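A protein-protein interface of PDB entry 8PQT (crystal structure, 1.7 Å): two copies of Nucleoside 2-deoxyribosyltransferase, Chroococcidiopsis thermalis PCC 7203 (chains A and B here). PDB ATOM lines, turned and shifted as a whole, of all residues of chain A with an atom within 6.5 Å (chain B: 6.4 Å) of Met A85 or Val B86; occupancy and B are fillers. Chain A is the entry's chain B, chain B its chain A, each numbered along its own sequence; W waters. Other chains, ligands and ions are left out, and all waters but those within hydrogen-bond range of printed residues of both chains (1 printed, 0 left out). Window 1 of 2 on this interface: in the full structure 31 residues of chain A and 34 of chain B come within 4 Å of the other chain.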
ATOM      1  N   ALA A  73      -1.576   7.775   3.131  1.00  0.00           N
ATOM      2  CA  ALA A  73      -2.680   7.029   2.543  1.00  0.00           C
ATOM      3  C   ALA A  73      -3.432   7.905   1.553  1.00  0.00           C
ATOM      4  O   ALA A  73      -3.999   8.930   1.943  1.00  0.00           O
ATOM      5  CB  ALA A  73      -3.630   6.545   3.638  1.00  0.00           C
ATOM      6  N   VAL A  74      -3.424   7.493   0.290  1.00  0.00           N
ATOM      7  CA  VAL A  74      -4.201   8.149  -0.755  1.00  0.00           C
ATOM      8  C   VAL A  74      -5.643   7.662  -0.620  1.00  0.00           C
ATOM      9  O   VAL A  74      -5.939   6.515  -0.936  1.00  0.00           O
ATOM     10  CB  VAL A  74      -3.636   7.860  -2.146  1.00  0.00           C
ATOM     11  CG1 VAL A  74      -4.521   8.441  -3.198  1.00  0.00           C
ATOM     12  CG2 VAL A  74      -2.186   8.421  -2.266  1.00  0.00           C
ATOM     13  N   VAL A  75      -6.543   8.551  -0.188  1.00  0.00           N
ATOM     14  CA  VAL A  75      -7.908   8.154   0.144  1.00  0.00           C
ATOM     15  C   VAL A  75      -8.875   8.867  -0.782  1.00  0.00           C
ATOM     16  O   VAL A  75     -10.015   9.169  -0.403  1.00  0.00           O
ATOM     17  CB  VAL A  75      -8.219   8.417   1.622  1.00  0.00           C
ATOM     18  CG1 VAL A  75      -7.246   7.627   2.497  1.00  0.00           C
ATOM     19  CG2 VAL A  75      -8.145   9.882   1.971  1.00  0.00           C
ATOM     20  N   PRO A  80     -13.210   5.564  -0.431  1.00  0.00           N
ATOM     21  CA  PRO A  80     -11.779   5.233  -0.474  1.00  0.00           C
ATOM     22  C   PRO A  80     -11.530   3.739  -0.647  1.00  0.00           C
ATOM     23  O   PRO A  80     -12.372   2.888  -0.354  1.00  0.00           O
ATOM     24  CB  PRO A  80     -11.267   5.751   0.871  1.00  0.00           C
ATOM     25  CG  PRO A  80     -12.239   6.878   1.209  1.00  0.00           C
ATOM     26  CD  PRO A  80     -13.563   6.419   0.709  1.00  0.00           C
ATOM     27  N   ASP A  81     -10.341   3.417  -1.156  1.00  0.00           N
ATOM     28  CA  ASP A  81     -10.003   2.039  -1.484  1.00  0.00           C
ATOM     29  C   ASP A  81      -9.980   1.117  -0.260  1.00  0.00           C
ATOM     30  O   ASP A  81      -9.337   1.407   0.743  1.00  0.00           O
ATOM     31  CB  ASP A  81      -8.632   1.999  -2.153  1.00  0.00           C
ATOM     32  CG  ASP A  81      -8.253   0.612  -2.592  1.00  0.00           C
ATOM     33  OD1 ASP A  81      -8.699   0.157  -3.681  1.00  0.00           O
ATOM     34  OD2 ASP A  81      -7.512  -0.032  -1.836  1.00  0.00           O
ATOM     35  N   GLU A  82     -10.595  -0.059  -0.397  1.00  0.00           N
ATOM     36  CA  GLU A  82     -10.731  -0.964   0.751  1.00  0.00           C
ATOM     37  C   GLU A  82      -9.384  -1.527   1.213  1.00  0.00           C
ATOM     38  O   GLU A  82      -9.173  -1.726   2.412  1.00  0.00           O
ATOM     39  CB  GLU A  82     -11.723  -2.089   0.380  1.00  0.00           C
ATOM     40  CG  GLU A  82     -11.289  -2.996  -0.722  1.00  0.00           C
ATOM     41  CD  GLU A  82     -11.764  -2.564  -2.110  1.00  0.00           C
ATOM     42  OE1 GLU A  82     -11.911  -1.343  -2.343  1.00  0.00           O
ATOM     43  OE2 GLU A  82     -11.924  -3.472  -2.956  1.00  0.00           O
ATOM     44  N   GLY A  83      -8.457  -1.763   0.292  1.00  0.00           N
ATOM     45  CA  GLY A  83      -7.136  -2.226   0.684  1.00  0.00           C
ATOM     46  C   GLY A  83      -6.350  -1.162   1.427  1.00  0.00           C
ATOM     47  O   GLY A  83      -5.742  -1.417   2.479  1.00  0.00           O
ATOM     48  N   VAL A  84      -6.375   0.060   0.905  1.00  0.00           N
ATOM     49  CA  VAL A  84      -5.763   1.167   1.618  1.00  0.00           C
ATOM     50  C   VAL A  84      -6.343   1.287   3.018  1.00  0.00           C
ATOM     51  O   VAL A  84      -5.618   1.504   3.997  1.00  0.00           O
ATOM     52  CB  VAL A  84      -5.943   2.472   0.815  1.00  0.00           C
ATOM     53  CG1 VAL A  84      -5.444   3.646   1.627  1.00  0.00           C
ATOM     54  CG2 VAL A  84      -5.264   2.378  -0.529  1.00  0.00           C
ATOM     55  N   MET A  85      -7.667   1.179   3.139  1.00  0.00           N
ATOM     56  CA  MET A  85      -8.295   1.252   4.463  1.00  0.00           C
ATOM     57  C   MET A  85      -7.775   0.183   5.426  1.00  0.00           C
ATOM     58  O   MET A  85      -7.598   0.472   6.616  1.00  0.00           O
ATOM     59  CB  MET A  85      -9.823   1.186   4.343  1.00  0.00           C
ATOM     60  CG  MET A  85     -10.345   2.295   3.435  1.00  0.00           C
ATOM     61  SD  MET A  85     -10.316   3.858   4.355  1.00  0.00           S
ATOM     62  CE  MET A  85      -8.842   4.645   3.573  1.00  0.00           C
ATOM     63  N   VAL A  86      -7.589  -1.054   4.961  1.00  0.00           N
ATOM     64  CA  VAL A  86      -7.052  -2.108   5.826  1.00  0.00           C
ATOM     65  C   VAL A  86      -5.670  -1.713   6.322  1.00  0.00           C
ATOM     66  O   VAL A  86      -5.380  -1.743   7.521  1.00  0.00           O
ATOM     67  CB  VAL A  86      -7.025  -3.452   5.083  1.00  0.00           C
ATOM     68  CG1 VAL A  86      -6.289  -4.496   5.853  1.00  0.00           C
ATOM     69  CG2 VAL A  86      -8.466  -3.938   4.868  1.00  0.00           C
ATOM     70  N   GLU A  87      -4.833  -1.243   5.407  1.00  0.00           N
ATOM     71  CA  GLU A  87      -3.492  -0.774   5.795  1.00  0.00           C
ATOM     72  C   GLU A  87      -3.546   0.405   6.758  1.00  0.00           C
ATOM     73  O   GLU A  87      -2.751   0.470   7.701  1.00  0.00           O
ATOM     74  CB  GLU A  87      -2.690  -0.429   4.536  1.00  0.00           C
ATOM     75  CG  GLU A  87      -2.477  -1.615   3.646  1.00  0.00           C
ATOM     76  CD  GLU A  87      -1.900  -1.285   2.288  1.00  0.00           C
ATOM     77  OE1 GLU A  87      -2.167  -0.167   1.755  1.00  0.00           O
ATOM     78  OE2 GLU A  87      -1.302  -2.205   1.706  1.00  0.00           O
ATOM     79  N   LEU A  88      -4.467   1.357   6.548  1.00  0.00           N
ATOM     80  CA  LEU A  88      -4.611   2.474   7.468  1.00  0.00           C
ATOM     81  C   LEU A  88      -4.958   1.983   8.873  1.00  0.00           C
ATOM     82  O   LEU A  88      -4.392   2.450   9.868  1.00  0.00           O
ATOM     83  CB  LEU A  88      -5.688   3.424   6.943  1.00  0.00           C
ATOM     84  CG  LEU A  88      -6.127   4.578   7.813  1.00  0.00           C
ATOM     85  CD1 LEU A  88      -4.945   5.483   8.128  1.00  0.00           C
ATOM     86  CD2 LEU A  88      -7.250   5.341   7.097  1.00  0.00           C
ATOM     87  N   GLY A  89      -5.901   1.044   8.967  1.00  0.00           N
ATOM     88  CA  GLY A  89      -6.260   0.483  10.261  1.00  0.00           C
ATOM     89  C   GLY A  89      -5.089  -0.212  10.948  1.00  0.00           C
ATOM     90  O   GLY A  89      -4.906  -0.070  12.166  1.00  0.00           O
ATOM     91  N   MET A  90      -4.307  -0.990  10.183  1.00  0.00           N
ATOM     92  CA  MET A  90      -3.105  -1.619  10.733  1.00  0.00           C
ATOM     93  C   MET A  90      -2.140  -0.563  11.251  1.00  0.00           C
ATOM     94  O   MET A  90      -1.614  -0.679  12.368  1.00  0.00           O
ATOM     95  CB  MET A  90      -2.411  -2.472   9.683  1.00  0.00           C
ATOM     96  CG  MET A  90      -3.235  -3.582   9.033  1.00  0.00           C
ATOM     97  SD  MET A  90      -2.260  -4.306   7.702  1.00  0.00           S
ATOM     98  CE  MET A  90      -3.108  -5.891   7.516  1.00  0.00           C
ATOM     99  N   ILE A  92      -2.819   2.545  12.246  1.00  0.00           N
ATOM    100  CA  ILE A  92      -3.339   3.148  13.462  1.00  0.00           C
ATOM    101  C   ILE A  92      -3.057   2.245  14.663  1.00  0.00           C
ATOM    102  O   ILE A  92      -2.529   2.696  15.693  1.00  0.00           O
ATOM    103  CB  ILE A  92      -4.841   3.453  13.319  1.00  0.00           C
ATOM    104  CG1 ILE A  92      -5.075   4.569  12.289  1.00  0.00           C
ATOM    105  CG2 ILE A  92      -5.427   3.842  14.652  1.00  0.00           C
ATOM    106  CD1 ILE A  92      -6.518   4.613  11.746  1.00  0.00           C
ATOM    107  N   LEU A 100      -3.032  11.601   5.672  1.00  0.00           N
ATOM    108  CA  LEU A 100      -4.052  11.310   4.677  1.00  0.00           C
ATOM    109  C   LEU A 100      -3.956  12.296   3.523  1.00  0.00           C
ATOM    110  O   LEU A 100      -3.711  13.486   3.731  1.00  0.00           O
ATOM    111  CB  LEU A 100      -5.462  11.378   5.276  1.00  0.00           C
ATOM    112  CG  LEU A 100      -5.703  10.524   6.542  1.00  0.00           C
ATOM    113  CD1 LEU A 100      -7.092  10.716   7.041  1.00  0.00           C
ATOM    114  CD2 LEU A 100      -5.420   9.067   6.220  1.00  0.00           C
ATOM    115  N   MET A 119     -14.463   7.217  10.993  1.00  0.00           N
ATOM    116  CA  MET A 119     -13.502   6.223  11.543  1.00  0.00           C
ATOM    117  C   MET A 119     -12.124   6.430  10.884  1.00  0.00           C
ATOM    118  O   MET A 119     -11.171   5.904  11.404  1.00  0.00           O
ATOM    119  CB  MET A 119     -13.950   4.784  11.317  1.00  0.00           C
ATOM    120  CG  MET A 119     -13.108   3.768  12.053  1.00  0.00           C
ATOM    121  SD  MET A 119     -13.305   3.975  13.839  1.00  0.00           S
ATOM    122  CE  MET A 119     -12.373   2.570  14.441  1.00  0.00           C
ATOM    123  N   LEU A 120     -12.092   6.979   9.657  1.00  0.00           N
ATOM    124  CA  LEU A 120     -10.790   7.144   9.014  1.00  0.00           C
ATOM    125  C   LEU A 120      -9.877   8.074   9.804  1.00  0.00           C
ATOM    126  O   LEU A 120      -8.656   8.010   9.633  1.00  0.00           O
ATOM    127  CB  LEU A 120     -10.969   7.659   7.584  1.00  0.00           C
ATOM    128  CG  LEU A 120     -11.129   6.581   6.517  1.00  0.00           C
ATOM    129  CD1 LEU A 120     -12.319   5.658   6.809  1.00  0.00           C
ATOM    130  CD2 LEU A 120     -11.296   7.268   5.155  1.00  0.00           C
ATOM    131  N   ALA A 122      -9.625   8.198  13.129  1.00  0.00           N
ATOM    132  CA  ALA A 122      -9.510   7.708  14.494  1.00  0.00           C
ATOM    133  C   ALA A 122      -8.086   7.783  15.003  1.00  0.00           C
ATOM    134  O   ALA A 122      -7.881   7.844  16.216  1.00  0.00           O
ATOM    135  CB  ALA A 122     -10.008   6.266  14.591  1.00  0.00           C
ATOM    136  N   ASP B  81     -17.209  -1.656   2.909  1.00  0.00           N
ATOM    137  CA  ASP B  81     -17.295  -0.361   3.570  1.00  0.00           C
ATOM    138  C   ASP B  81     -15.947   0.102   4.117  1.00  0.00           C
ATOM    139  O   ASP B  81     -15.257  -0.649   4.799  1.00  0.00           O
ATOM    140  CB  ASP B  81     -18.305  -0.433   4.715  1.00  0.00           C
ATOM    141  CG  ASP B  81     -18.419   0.866   5.437  1.00  0.00           C
ATOM    142  OD1 ASP B  81     -19.172   1.733   4.952  1.00  0.00           O
ATOM    143  OD2 ASP B  81     -17.710   1.046   6.455  1.00  0.00           O
ATOM    144  N   GLU B  82     -15.604   1.367   3.879  1.00  0.00           N
ATOM    145  CA  GLU B  82     -14.269   1.846   4.248  1.00  0.00           C
ATOM    146  C   GLU B  82     -14.045   1.860   5.766  1.00  0.00           C
ATOM    147  O   GLU B  82     -12.930   1.581   6.224  1.00  0.00           O
ATOM    148  CB  GLU B  82     -14.030   3.227   3.625  1.00  0.00           C
ATOM    149  CG  GLU B  82     -14.931   4.339   4.173  1.00  0.00           C
ATOM    150  CD  GLU B  82     -16.237   4.539   3.415  1.00  0.00           C
ATOM    151  OE1 GLU B  82     -16.747   3.605   2.742  1.00  0.00           O
ATOM    152  OE2 GLU B  82     -16.709   5.676   3.502  1.00  0.00           O
ATOM    153  N   GLY B  83     -15.078   2.145   6.564  1.00  0.00           N
ATOM    154  CA  GLY B  83     -14.917   2.112   8.009  1.00  0.00           C
ATOM    155  C   GLY B  83     -14.754   0.703   8.551  1.00  0.00           C
ATOM    156  O   GLY B  83     -13.943   0.467   9.450  1.00  0.00           O
ATOM    157  N   VAL B  84     -15.523  -0.255   8.012  1.00  0.00           N
ATOM    158  CA  VAL B  84     -15.322  -1.662   8.367  1.00  0.00           C
ATOM    159  C   VAL B  84     -13.897  -2.092   8.074  1.00  0.00           C
ATOM    160  O   VAL B  84     -13.273  -2.832   8.837  1.00  0.00           O
ATOM    161  CB  VAL B  84     -16.326  -2.558   7.625  1.00  0.00           C
ATOM    162  CG1 VAL B  84     -16.029  -4.053   7.933  1.00  0.00           C
ATOM    163  CG2 VAL B  84     -17.760  -2.171   8.039  1.00  0.00           C
ATOM    164  N   MET B  85     -13.368  -1.637   6.945  1.00  0.00           N
ATOM    165  CA  MET B  85     -12.042  -2.016   6.499  1.00  0.00           C
ATOM    166  C   MET B  85     -10.982  -1.520   7.478  1.00  0.00           C
ATOM    167  O   MET B  85     -10.023  -2.239   7.783  1.00  0.00           O
ATOM    168  CB  MET B  85     -11.851  -1.406   5.120  1.00  0.00           C
ATOM    169  CG  MET B  85     -12.366  -2.223   3.929  1.00  0.00           C
ATOM    170  SD  MET B  85     -12.242  -3.981   3.859  1.00  0.00           S
ATOM    171  CE  MET B  85     -13.660  -4.671   4.758  1.00  0.00           C
ATOM    172  N   VAL B  86     -11.118  -0.272   7.948  1.00  0.00           N
ATOM    173  CA  VAL B  86     -10.193   0.267   8.961  1.00  0.00           C
ATOM    174  C   VAL B  86     -10.206  -0.621  10.204  1.00  0.00           C
ATOM    175  O   VAL B  86      -9.156  -0.965  10.773  1.00  0.00           O
ATOM    176  CB  VAL B  86     -10.561   1.720   9.308  1.00  0.00           C
ATOM    177  CG1 VAL B  86      -9.792   2.197  10.559  1.00  0.00           C
ATOM    178  CG2 VAL B  86     -10.292   2.649   8.087  1.00  0.00           C
ATOM    179  N   GLU B  87     -11.402  -0.985  10.653  1.00  0.00           N
ATOM    180  CA  GLU B  87     -11.541  -1.824  11.845  1.00  0.00           C
ATOM    181  C   GLU B  87     -10.935  -3.196  11.628  1.00  0.00           C
ATOM    182  O   GLU B  87     -10.260  -3.734  12.516  1.00  0.00           O
ATOM    183  CB  GLU B  87     -13.032  -1.916  12.233  1.00  0.00           C
ATOM    184  CG  GLU B  87     -13.595  -0.611  12.782  1.00  0.00           C
ATOM    185  CD  GLU B  87     -15.102  -0.555  12.847  1.00  0.00           C
ATOM    186  OE1 GLU B  87     -15.759  -1.303  12.098  1.00  0.00           O
ATOM    187  OE2 GLU B  87     -15.611   0.308  13.592  1.00  0.00           O
ATOM    188  N   LEU B  88     -11.129  -3.764  10.436  1.00  0.00           N
ATOM    189  CA  LEU B  88     -10.541  -5.047  10.102  1.00  0.00           C
ATOM    190  C   LEU B  88      -9.027  -4.973  10.168  1.00  0.00           C
ATOM    191  O   LEU B  88      -8.373  -5.861  10.737  1.00  0.00           O
ATOM    192  CB  LEU B  88     -11.005  -5.472   8.724  1.00  0.00           C
ATOM    193  CG  LEU B  88     -10.402  -6.722   8.117  1.00  0.00           C
ATOM    194  CD1 LEU B  88     -10.704  -7.952   8.999  1.00  0.00           C
ATOM    195  CD2 LEU B  88     -10.947  -6.896   6.714  1.00  0.00           C
ATOM    196  N   GLY B  89      -8.443  -3.900   9.619  1.00  0.00           N
ATOM    197  CA  GLY B  89      -6.993  -3.776   9.675  1.00  0.00           C
ATOM    198  C   GLY B  89      -6.488  -3.647  11.098  1.00  0.00           C
ATOM    199  O   GLY B  89      -5.416  -4.159  11.444  1.00  0.00           O
ATOM    200  N   MET B  90      -7.225  -2.921  11.924  1.00  0.00           N
ATOM    201  CA  MET B  90      -6.927  -2.768  13.340  1.00  0.00           C
ATOM    202  C   MET B  90      -6.921  -4.140  14.018  1.00  0.00           C
ATOM    203  O   MET B  90      -5.990  -4.526  14.740  1.00  0.00           O
ATOM    204  CB  MET B  90      -8.027  -1.881  13.883  1.00  0.00           C
ATOM    205  CG  MET B  90      -7.754  -0.381  13.838  1.00  0.00           C
ATOM    206  SD  MET B  90      -9.134   0.490  14.577  1.00  0.00           S
ATOM    207  CE  MET B  90      -8.540   2.187  14.353  1.00  0.00           C
ATOM    208  N   ALA B  91      -7.945  -4.930  13.723  1.00  0.00           N
ATOM    209  CA  ALA B  91      -8.062  -6.257  14.319  1.00  0.00           C
ATOM    210  C   ALA B  91      -6.931  -7.174  13.887  1.00  0.00           C
ATOM    211  O   ALA B  91      -6.417  -7.946  14.701  1.00  0.00           O
ATOM    212  CB  ALA B  91      -9.412  -6.881  13.953  1.00  0.00           C
HETATM  213  O   HOH W   1     -13.367   0.740   1.421  1.00  0.00           O
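Of the 11 printed residues of chain B, 6 touch a printed residue of chain A. Hydrophobic or aromatic side chains of chain B within 4 Å of the printed part of chain A: Met B85, Val B86 and Met B90. Printed residues of chain A that touch a printed residue of chain B: Glu A82, Met A85, Val A86, Gly A89, Met A90, Ile A92, Met A119 and Leu A120. Among the printed residues, no Asp or Glu carboxylate lies within 4 Å of a Lys or Arg side-chain nitrogen of the other chain.
Water W1 lies within hydrogen-bond range of O of Pro A80 (3.0 Å), N of Glu B82 (3.4 Å) and N of Glu A82 (3.4 Å).
Met A85 touches its own counterpart, Met B85. Gly A89 touches its own counterpart, Gly B89. Gly A89 touches Met B90, and with the chains exchanged Met A90 touches Gly B89. Met A90 touches its own counterpart, Met B90. Positions printed for both chains: 81, 82, 83, 84, 85, 86, 87, 88, 89 and 90. Of the 17 pairs that touch across the chains among the printed residues, 11 have their exchanged pair printed and touching as well.
Of chain B, only Glu B82 (3.7 Å), Met B85 (3.4 Å) and Val B86 (3.5 Å) come within 4 Å of Met A85. Of the printed residues of chain A, Val B86 touches Met A85 (3.5 Å), Gly A89 (3.3 Å), Met A119 (3.96 Å) and Leu A120 (3.8 Å). Of the printed residues of chain A, Met B90 touches Gly A89, Met A90, Ile A92 and Met A119. Of the printed residues of chain B, Met A90 touches Gly B89 and Met B90. Val B84 touches none of the printed residues of chain A. The nearest residue of chain B that does not touch Met A85 is Gly B89 (5.3 Å). The nearest printed residue of chain B that does not touch Glu A82 is Glu B82 (5.7 Å).
Among the printed residues, pairs that only touch across the chains: Glu A82 with Met B85 (3.6 Å), Met A85 with Glu B82 (3.7 Å), Met A85 with Met B85 (3.4 Å), Met A85 with Val B86 (3.5 Å), Val A86 with Met B85 (3.6 Å), Val A86 with Gly B89 (3.4 Å), Gly A89 with Val B86 (3.3 Å), Gly A89 with Gly B89 (3.7 Å), Gly A89 with Met B90 (3.3 Å), Met A90 with Gly B89 (3.3 Å), Met A90 with Met B90 (3.9 Å), Ile A92 with Met B90 (3.5 Å), Met A119 with Val B86 (3.96 Å), Met A119 with Glu B87 (3.8 Å), Met A119 with Met B90 (3.9 Å), Leu A120 with Glu B82 (3.9 Å) and Leu A120 with Val B86 (3.8 Å).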
